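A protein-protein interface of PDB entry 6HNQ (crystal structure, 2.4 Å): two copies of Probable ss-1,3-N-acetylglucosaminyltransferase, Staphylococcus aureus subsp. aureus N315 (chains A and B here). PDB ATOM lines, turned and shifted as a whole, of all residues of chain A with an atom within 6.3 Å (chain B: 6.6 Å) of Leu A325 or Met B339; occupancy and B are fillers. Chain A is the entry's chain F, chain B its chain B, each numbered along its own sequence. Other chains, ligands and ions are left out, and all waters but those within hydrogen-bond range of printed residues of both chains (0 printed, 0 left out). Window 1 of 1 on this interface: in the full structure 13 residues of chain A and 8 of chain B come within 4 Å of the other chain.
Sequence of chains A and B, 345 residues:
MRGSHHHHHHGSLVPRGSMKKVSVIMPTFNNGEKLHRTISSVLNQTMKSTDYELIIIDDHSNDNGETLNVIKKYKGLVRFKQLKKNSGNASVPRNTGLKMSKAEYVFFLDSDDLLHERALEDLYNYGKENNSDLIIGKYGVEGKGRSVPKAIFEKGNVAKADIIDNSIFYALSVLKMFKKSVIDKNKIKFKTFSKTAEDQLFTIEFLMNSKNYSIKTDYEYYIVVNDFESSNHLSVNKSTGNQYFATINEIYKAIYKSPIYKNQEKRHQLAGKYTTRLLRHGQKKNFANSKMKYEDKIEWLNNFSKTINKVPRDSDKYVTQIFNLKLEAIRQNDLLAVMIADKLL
Ile A322 touches Lys B343 (O to NZ, 3.7 Å).
Asn A324 touches Met B339 (ND2 to CE, 3.5 Å).
CD2 of Leu B336 touches CD1 of Leu A325 (3.9 Å).
Leu A325 touches Met B339.
CD2 of Leu A325 touches CG1 of Ile B340, 3.5 Å away.
Met B339 touches Glu A328.
Leu B336 touches Ala A329 (CD2 to N, 3.7 Å).
Ala A337 touches Leu B336.
Ile A340 touches Ile B340 (CG2 to CD1, 3.8 Å).
Leu B344 touches Leu A344 (CD2 to CD2, 3.6 Å).
The side-chain amide oxygen (OD1) of Asn B289 lies within hydrogen-bond range of the side-chain amide nitrogen (ND2) of Asn A324 (2.4 Å).
OD1 of Asn A324 lies within hydrogen-bond range of NZ of Lys B343, 2.8 Å away.
Ile A340 touches its own counterpart, Ile B340.
Leu B344 touches its own counterpart, Leu A344.
5 positions are printed for both chains.
The backbone carbonyl oxygen of Met B339 is in hydrogen-bond range of the side-chain amide nitrogen of Asn B289, at 2.9 Å.
OD1 of Asp B334 lies within hydrogen-bond range of N of Leu B336 (3.2 Å).
The backbone carbonyl oxygen of Gln A321 sits close to the side-chain amide oxygen of Asn A324 (2.9 Å).
Of chain B, only Leu B336 (3.9 Å), Met B339 (3.6 Å) and Ile B340 (3.5 Å) come within 4 Å of Leu A325.
Met B339 touches just these residues of chain A: Asn A324 (3.5 Å), Leu A325 (3.6 Å) and Glu A328 (3.9 Å).
Of the printed residues of chain B, Glu A328 touches Met B339.
Of the printed residues of chain B, Ala A329 touches Leu B336.
Printed residues of chain A within 4 Å of Lys B343: Gln A321, Ile A322 and Asn A324.
Of the printed residues of chain B, Ile A340 touches Ile B340.
The nearest residue of chain B that does not touch Leu A325 is Lys B343 (4.3 Å).
The nearest printed residue of chain B that does not touch Ile A340 is Leu B344 (6.3 Å).
Of the 15 printed residues of chain B, 6 touch a printed residue of chain A.
Printed residues of chain B that touch a printed residue of chain A: Asn B289, Leu B336, Met B339, Ile B340, Lys B343 and Leu B344.
Hydrophobic or aromatic side chains of chain B within 4 Å of the printed part of chain A: Leu B336, Met B339, Ile B340 and Leu B344.
Along chain B the printed residues that touch a printed residue of chain A span positions 289 to 344.
Printed residues of chain A that touch a printed residue of chain B: Gln A321, Ile A322, Asn A324, Leu A325, Glu A328, Ala A329, Ala A337, Ile A340 and Leu A344.
Hydrophobic or aromatic side chains of chain A that line the printed part of chain B: Leu A325, Ala A337, Ile A340 and Leu A344.
Among the printed residues, 14 pairs touch across the chains.
Among the printed residues, no Asp or Glu carboxylate lies within 4 Å of a Lys or Arg side-chain nitrogen of the other chain.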
ATOM      1  N   GLN A 321      -2.891  -5.597  16.525  1.00  0.00           N
ATOM      2  CA  GLN A 321      -1.815  -6.031  15.591  1.00  0.00           C
ATOM      3  C   GLN A 321      -0.833  -4.900  15.290  1.00  0.00           C
ATOM      4  O   GLN A 321       0.314  -5.226  15.010  1.00  0.00           O
ATOM      5  CB  GLN A 321      -2.410  -6.659  14.334  1.00  0.00           C
ATOM      6  CG  GLN A 321      -2.741  -8.145  14.522  1.00  0.00           C
ATOM      7  CD  GLN A 321      -1.712  -8.941  15.304  1.00  0.00           C
ATOM      8  OE1 GLN A 321      -1.914  -9.294  16.466  1.00  0.00           O
ATOM      9  NE2 GLN A 321      -0.603  -9.284  14.663  1.00  0.00           N
ATOM     10  N   ILE A 322      -1.214  -3.629  15.369  1.00  0.00           N
ATOM     11  CA  ILE A 322      -0.272  -2.486  15.141  1.00  0.00           C
ATOM     12  C   ILE A 322       0.951  -2.631  16.057  1.00  0.00           C
ATOM     13  O   ILE A 322       2.023  -2.124  15.676  1.00  0.00           O
ATOM     14  CB  ILE A 322      -0.943  -1.112  15.329  1.00  0.00           C
ATOM     15  CG1 ILE A 322      -1.531  -0.932  16.725  1.00  0.00           C
ATOM     16  CG2 ILE A 322      -2.005  -0.881  14.262  1.00  0.00           C
ATOM     17  CD1 ILE A 322      -1.830   0.518  17.057  1.00  0.00           C
ATOM     18  N   PHE A 323       0.815  -3.301  17.205  1.00  0.00           N
ATOM     19  CA  PHE A 323       1.891  -3.427  18.215  1.00  0.00           C
ATOM     20  C   PHE A 323       2.691  -4.717  18.031  1.00  0.00           C
ATOM     21  O   PHE A 323       3.569  -4.987  18.887  1.00  0.00           O
ATOM     22  CB  PHE A 323       1.309  -3.373  19.621  1.00  0.00           C
ATOM     23  CG  PHE A 323       0.701  -2.048  19.980  1.00  0.00           C
ATOM     24  CD1 PHE A 323       1.485  -0.906  20.008  1.00  0.00           C
ATOM     25  CD2 PHE A 323      -0.643  -1.940  20.287  1.00  0.00           C
ATOM     26  CE1 PHE A 323       0.935   0.315  20.377  1.00  0.00           C
ATOM     27  CE2 PHE A 323      -1.178  -0.711  20.599  1.00  0.00           C
ATOM     28  CZ  PHE A 323      -0.402   0.422  20.610  1.00  0.00           C
ATOM     29  N   ASN A 324       2.432  -5.476  16.965  1.00  0.00           N
ATOM     30  CA  ASN A 324       3.049  -6.815  16.770  1.00  0.00           C
ATOM     31  C   ASN A 324       4.579  -6.665  16.767  1.00  0.00           C
ATOM     32  O   ASN A 324       5.252  -7.472  17.430  1.00  0.00           O
ATOM     33  CB  ASN A 324       2.516  -7.507  15.505  1.00  0.00           C
ATOM     34  CG  ASN A 324       3.051  -6.944  14.198  1.00  0.00           C
ATOM     35  OD1 ASN A 324       2.972  -5.735  13.927  1.00  0.00           O
ATOM     36  ND2 ASN A 324       3.543  -7.842  13.368  1.00  0.00           N
ATOM     37  N   LEU A 325       5.112  -5.677  16.043  1.00  0.00           N
ATOM     38  CA  LEU A 325       6.577  -5.481  15.896  1.00  0.00           C
ATOM     39  C   LEU A 325       7.162  -5.007  17.229  1.00  0.00           C
ATOM     40  O   LEU A 325       8.149  -5.615  17.700  1.00  0.00           O
ATOM     41  CB  LEU A 325       6.847  -4.468  14.779  1.00  0.00           C
ATOM     42  CG  LEU A 325       8.296  -4.016  14.654  1.00  0.00           C
ATOM     43  CD1 LEU A 325       9.222  -5.201  14.418  1.00  0.00           C
ATOM     44  CD2 LEU A 325       8.430  -2.984  13.549  1.00  0.00           C
ATOM     45  N   LYS A 326       6.557  -3.995  17.842  1.00  0.00           N
ATOM     46  CA  LYS A 326       7.078  -3.444  19.115  1.00  0.00           C
ATOM     47  C   LYS A 326       7.136  -4.554  20.166  1.00  0.00           C
ATOM     48  O   LYS A 326       8.161  -4.658  20.870  1.00  0.00           O
ATOM     49  CB  LYS A 326       6.221  -2.297  19.638  1.00  0.00           C
ATOM     50  CG  LYS A 326       6.801  -1.656  20.885  1.00  0.00           C
ATOM     51  CD  LYS A 326       6.297  -0.260  21.116  1.00  0.00           C
ATOM     52  CE  LYS A 326       7.053   0.444  22.218  1.00  0.00           C
ATOM     53  NZ  LYS A 326       6.460   1.757  22.523  1.00  0.00           N
ATOM     54  N   LEU A 327       6.067  -5.343  20.285  1.00  0.00           N
ATOM     55  CA  LEU A 327       6.011  -6.442  21.281  1.00  0.00           C
ATOM     56  C   LEU A 327       7.145  -7.435  21.002  1.00  0.00           C
ATOM     57  O   LEU A 327       7.841  -7.822  21.948  1.00  0.00           O
ATOM     58  CB  LEU A 327       4.649  -7.133  21.201  1.00  0.00           C
ATOM     59  CG  LEU A 327       4.472  -8.363  22.090  1.00  0.00           C
ATOM     60  CD1 LEU A 327       4.801  -8.031  23.517  1.00  0.00           C
ATOM     61  CD2 LEU A 327       3.052  -8.869  21.983  1.00  0.00           C
ATOM     62  N   GLU A 328       7.321  -7.834  19.742  1.00  0.00           N
ATOM     63  CA  GLU A 328       8.347  -8.842  19.391  1.00  0.00           C
ATOM     64  C   GLU A 328       9.729  -8.228  19.653  1.00  0.00           C
ATOM     65  O   GLU A 328      10.600  -8.944  20.169  1.00  0.00           O
ATOM     66  CB  GLU A 328       8.214  -9.318  17.947  1.00  0.00           C
ATOM     67  CG  GLU A 328       9.091 -10.522  17.654  1.00  0.00           C
ATOM     68  CD  GLU A 328       8.859 -11.709  18.568  1.00  0.00           C
ATOM     69  OE1 GLU A 328       7.679 -12.126  18.718  1.00  0.00           O
ATOM     70  OE2 GLU A 328       9.851 -12.219  19.133  1.00  0.00           O
ATOM     71  N   ALA A 329       9.912  -6.946  19.345  1.00  0.00           N
ATOM     72  CA  ALA A 329      11.179  -6.226  19.625  1.00  0.00           C
ATOM     73  C   ALA A 329      11.510  -6.321  21.123  1.00  0.00           C
ATOM     74  O   ALA A 329      12.678  -6.589  21.471  1.00  0.00           O
ATOM     75  CB  ALA A 329      11.065  -4.795  19.169  1.00  0.00           C
ATOM     76  N   ILE A 330      10.515  -6.118  21.987  1.00  0.00           N
ATOM     77  CA  ILE A 330      10.727  -6.167  23.461  1.00  0.00           C
ATOM     78  C   ILE A 330      11.080  -7.607  23.864  1.00  0.00           C
ATOM     79  O   ILE A 330      12.006  -7.793  24.679  1.00  0.00           O
ATOM     80  CB  ILE A 330       9.506  -5.603  24.202  1.00  0.00           C
ATOM     81  CG1 ILE A 330       9.353  -4.102  23.942  1.00  0.00           C
ATOM     82  CG2 ILE A 330       9.579  -5.918  25.682  1.00  0.00           C
ATOM     83  CD1 ILE A 330       7.970  -3.562  24.202  1.00  0.00           C
ATOM     84  N   ALA A 337      15.273  -2.307  17.325  1.00  0.00           N
ATOM     85  CA  ALA A 337      13.967  -2.747  16.793  1.00  0.00           C
ATOM     86  C   ALA A 337      12.846  -1.979  17.503  1.00  0.00           C
ATOM     87  O   ALA A 337      11.860  -1.613  16.827  1.00  0.00           O
ATOM     88  CB  ALA A 337      13.831  -4.238  16.922  1.00  0.00           C
ATOM     89  N   ILE A 340      12.820   1.508  16.018  1.00  0.00           N
ATOM     90  CA  ILE A 340      12.193   1.440  14.671  1.00  0.00           C
ATOM     91  C   ILE A 340      10.680   1.269  14.840  1.00  0.00           C
ATOM     92  O   ILE A 340       9.926   2.002  14.177  1.00  0.00           O
ATOM     93  CB  ILE A 340      12.828   0.320  13.834  1.00  0.00           C
ATOM     94  CG1 ILE A 340      14.278   0.657  13.474  1.00  0.00           C
ATOM     95  CG2 ILE A 340      11.990   0.040  12.596  1.00  0.00           C
ATOM     96  CD1 ILE A 340      15.123  -0.529  13.148  1.00  0.00           C
ATOM     97  N   ALA A 341      10.246   0.347  15.700  1.00  0.00           N
ATOM     98  CA  ALA A 341       8.809   0.082  15.930  1.00  0.00           C
ATOM     99  C   ALA A 341       8.107   1.403  16.277  1.00  0.00           C
ATOM    100  O   ALA A 341       7.024   1.669  15.721  1.00  0.00           O
ATOM    101  CB  ALA A 341       8.623  -0.947  17.019  1.00  0.00           C
ATOM    102  N   LEU A 344       7.564   3.738  13.403  1.00  0.00           N
ATOM    103  CA  LEU A 344       6.507   3.246  12.477  1.00  0.00           C
ATOM    104  C   LEU A 344       5.109   3.416  13.097  1.00  0.00           C
ATOM    105  O   LEU A 344       4.139   3.477  12.317  1.00  0.00           O
ATOM    106  CB  LEU A 344       6.781   1.785  12.122  1.00  0.00           C
ATOM    107  CG  LEU A 344       8.055   1.555  11.319  1.00  0.00           C
ATOM    108  CD1 LEU A 344       8.272   0.073  11.073  1.00  0.00           C
ATOM    109  CD2 LEU A 344       8.024   2.322  10.005  1.00  0.00           C
ATOM    110  N   ALA B 288       5.593 -12.981   8.575  1.00  0.00           N
ATOM    111  CA  ALA B 288       6.384 -12.339   9.647  1.00  0.00           C
ATOM    112  C   ALA B 288       5.466 -11.592  10.624  1.00  0.00           C
ATOM    113  O   ALA B 288       5.705 -11.703  11.832  1.00  0.00           O
ATOM    114  CB  ALA B 288       7.418 -11.411   9.051  1.00  0.00           C
ATOM    115  N   ASN B 289       4.469 -10.851  10.124  1.00  0.00           N
ATOM    116  CA  ASN B 289       3.558 -10.032  10.960  1.00  0.00           C
ATOM    117  C   ASN B 289       2.238 -10.783  11.214  1.00  0.00           C
ATOM    118  O   ASN B 289       1.305 -10.155  11.737  1.00  0.00           O
ATOM    119  CB  ASN B 289       3.332  -8.664  10.325  1.00  0.00           C
ATOM    120  CG  ASN B 289       4.569  -7.784  10.421  1.00  0.00           C
ATOM    121  OD1 ASN B 289       5.036  -7.456  11.511  1.00  0.00           O
ATOM    122  ND2 ASN B 289       5.123  -7.389   9.293  1.00  0.00           N
ATOM    123  N   LYS B 297       7.235 -19.436  12.931  1.00  0.00           N
ATOM    124  CA  LYS B 297       7.829 -18.311  12.165  1.00  0.00           C
ATOM    125  C   LYS B 297       9.334 -18.550  12.040  1.00  0.00           C
ATOM    126  O   LYS B 297       9.868 -18.367  10.950  1.00  0.00           O
ATOM    127  CB  LYS B 297       7.559 -16.975  12.853  1.00  0.00           C
ATOM    128  CG  LYS B 297       6.158 -16.438  12.651  1.00  0.00           C
ATOM    129  CD  LYS B 297       5.966 -15.124  13.410  1.00  0.00           C
ATOM    130  CE  LYS B 297       4.624 -14.500  13.120  1.00  0.00           C
ATOM    131  NZ  LYS B 297       4.477 -13.214  13.823  1.00  0.00           N
ATOM    132  N   ALA B 329      16.909  -9.152   4.695  1.00  0.00           N
ATOM    133  CA  ALA B 329      16.399  -9.645   5.997  1.00  0.00           C
ATOM    134  C   ALA B 329      16.312 -11.179   5.977  1.00  0.00           C
ATOM    135  O   ALA B 329      16.723 -11.823   6.966  1.00  0.00           O
ATOM    136  CB  ALA B 329      15.065  -9.024   6.281  1.00  0.00           C
ATOM    137  N   ASP B 334      16.646 -12.961   9.941  1.00  0.00           N
ATOM    138  CA  ASP B 334      16.350 -11.975  11.011  1.00  0.00           C
ATOM    139  C   ASP B 334      14.850 -11.666  10.978  1.00  0.00           C
ATOM    140  O   ASP B 334      14.425 -10.866  10.124  1.00  0.00           O
ATOM    141  CB  ASP B 334      17.213 -10.727  10.834  1.00  0.00           C
ATOM    142  CG  ASP B 334      17.084  -9.709  11.964  1.00  0.00           C
ATOM    143  OD1 ASP B 334      15.968  -9.540  12.484  1.00  0.00           O
ATOM    144  OD2 ASP B 334      18.113  -9.110  12.339  1.00  0.00           O
ATOM    145  N   LEU B 335      14.077 -12.270  11.880  1.00  0.00           N
ATOM    146  CA  LEU B 335      12.594 -12.154  11.861  1.00  0.00           C
ATOM    147  C   LEU B 335      12.192 -10.689  12.054  1.00  0.00           C
ATOM    148  O   LEU B 335      11.304 -10.236  11.326  1.00  0.00           O
ATOM    149  CB  LEU B 335      11.997 -13.035  12.956  1.00  0.00           C
ATOM    150  CG  LEU B 335      10.482 -13.020  13.067  1.00  0.00           C
ATOM    151  CD1 LEU B 335       9.823 -13.452  11.763  1.00  0.00           C
ATOM    152  CD2 LEU B 335      10.064 -13.974  14.200  1.00  0.00           C
ATOM    153  N   LEU B 336      12.816  -9.976  12.997  1.00  0.00           N
ATOM    154  CA  LEU B 336      12.465  -8.562  13.262  1.00  0.00           C
ATOM    155  C   LEU B 336      12.600  -7.746  11.974  1.00  0.00           C
ATOM    156  O   LEU B 336      11.715  -6.913  11.692  1.00  0.00           O
ATOM    157  CB  LEU B 336      13.362  -8.009  14.370  1.00  0.00           C
ATOM    158  CG  LEU B 336      12.925  -8.399  15.780  1.00  0.00           C
ATOM    159  CD1 LEU B 336      13.975  -8.058  16.818  1.00  0.00           C
ATOM    160  CD2 LEU B 336      11.619  -7.721  16.123  1.00  0.00           C
ATOM    161  N   ALA B 337      13.670  -7.975  11.220  1.00  0.00           N
ATOM    162  CA  ALA B 337      13.966  -7.200   9.993  1.00  0.00           C
ATOM    163  C   ALA B 337      12.916  -7.533   8.928  1.00  0.00           C
ATOM    164  O   ALA B 337      12.502  -6.602   8.195  1.00  0.00           O
ATOM    165  CB  ALA B 337      15.368  -7.470   9.519  1.00  0.00           C
ATOM    166  N   VAL B 338      12.469  -8.792   8.856  1.00  0.00           N
ATOM    167  CA  VAL B 338      11.411  -9.181   7.879  1.00  0.00           C
ATOM    168  C   VAL B 338      10.105  -8.494   8.284  1.00  0.00           C
ATOM    169  O   VAL B 338       9.419  -7.956   7.398  1.00  0.00           O
ATOM    170  CB  VAL B 338      11.246 -10.700   7.751  1.00  0.00           C
ATOM    171  CG1 VAL B 338      10.176 -11.041   6.737  1.00  0.00           C
ATOM    172  CG2 VAL B 338      12.551 -11.378   7.374  1.00  0.00           C
ATOM    173  N   MET B 339       9.792  -8.483   9.581  1.00  0.00           N
ATOM    174  CA  MET B 339       8.582  -7.815  10.102  1.00  0.00           C
ATOM    175  C   MET B 339       8.624  -6.340   9.696  1.00  0.00           C
ATOM    176  O   MET B 339       7.610  -5.823   9.186  1.00  0.00           O
ATOM    177  CB  MET B 339       8.492  -7.927  11.627  1.00  0.00           C
ATOM    178  CG  MET B 339       8.178  -9.318  12.119  1.00  0.00           C
ATOM    179  SD  MET B 339       8.300  -9.453  13.916  1.00  0.00           S
ATOM    180  CE  MET B 339       6.745  -8.694  14.392  1.00  0.00           C
ATOM    181  N   ILE B 340       9.767  -5.685   9.915  1.00  0.00           N
ATOM    182  CA  ILE B 340       9.933  -4.245   9.591  1.00  0.00           C
ATOM    183  C   ILE B 340       9.817  -4.066   8.070  1.00  0.00           C
ATOM    184  O   ILE B 340       9.079  -3.156   7.625  1.00  0.00           O
ATOM    185  CB  ILE B 340      11.259  -3.710  10.145  1.00  0.00           C
ATOM    186  CG1 ILE B 340      11.249  -3.679  11.672  1.00  0.00           C
ATOM    187  CG2 ILE B 340      11.559  -2.335   9.553  1.00  0.00           C
ATOM    188  CD1 ILE B 340      12.629  -3.707  12.272  1.00  0.00           C
ATOM    189  N   ALA B 341      10.507  -4.898   7.287  1.00  0.00           N
ATOM    190  CA  ALA B 341      10.480  -4.806   5.813  1.00  0.00           C
ATOM    191  C   ALA B 341       9.023  -4.815   5.330  1.00  0.00           C
ATOM    192  O   ALA B 341       8.668  -3.974   4.469  1.00  0.00           O
ATOM    193  CB  ALA B 341      11.268  -5.927   5.211  1.00  0.00           C
ATOM    194  N   ASP B 342       8.208  -5.723   5.884  1.00  0.00           N
ATOM    195  CA  ASP B 342       6.795  -5.891   5.465  1.00  0.00           C
ATOM    196  C   ASP B 342       5.999  -4.644   5.860  1.00  0.00           C
ATOM    197  O   ASP B 342       5.135  -4.223   5.074  1.00  0.00           O
ATOM    198  CB  ASP B 342       6.188  -7.172   6.046  1.00  0.00           C
ATOM    199  CG  ASP B 342       6.509  -8.430   5.271  1.00  0.00           C
ATOM    200  OD1 ASP B 342       6.814  -8.310   4.092  1.00  0.00           O
ATOM    201  OD2 ASP B 342       6.423  -9.531   5.854  1.00  0.00           O
ATOM    202  N   LYS B 343       6.285  -4.055   7.021  1.00  0.00           N
ATOM    203  CA  LYS B 343       5.582  -2.828   7.469  1.00  0.00           C
ATOM    204  C   LYS B 343       5.900  -1.681   6.507  1.00  0.00           C
ATOM    205  O   LYS B 343       5.006  -0.847   6.302  1.00  0.00           O
ATOM    206  CB  LYS B 343       5.959  -2.479   8.911  1.00  0.00           C
ATOM    207  CG  LYS B 343       5.420  -3.418   9.977  1.00  0.00           C
ATOM    208  CD  LYS B 343       4.040  -3.154  10.451  1.00  0.00           C
ATOM    209  CE  LYS B 343       3.760  -3.781  11.806  1.00  0.00           C
ATOM    210  NZ  LYS B 343       2.371  -3.506  12.263  1.00  0.00           N
ATOM    211  N   LEU B 344       7.091  -1.651   5.904  1.00  0.00           N
ATOM    212  CA  LEU B 344       7.508  -0.558   4.989  1.00  0.00           C
ATOM    213  C   LEU B 344       7.005  -0.807   3.559  1.00  0.00           C
ATOM    214  O   LEU B 344       6.907   0.167   2.804  1.00  0.00           O
ATOM    215  CB  LEU B 344       9.036  -0.425   5.023  1.00  0.00           C
ATOM    216  CG  LEU B 344       9.606   0.027   6.361  1.00  0.00           C
ATOM    217  CD1 LEU B 344      11.128   0.030   6.319  1.00  0.00           C
ATOM    218  CD2 LEU B 344       9.064   1.400   6.715  1.00  0.00           C
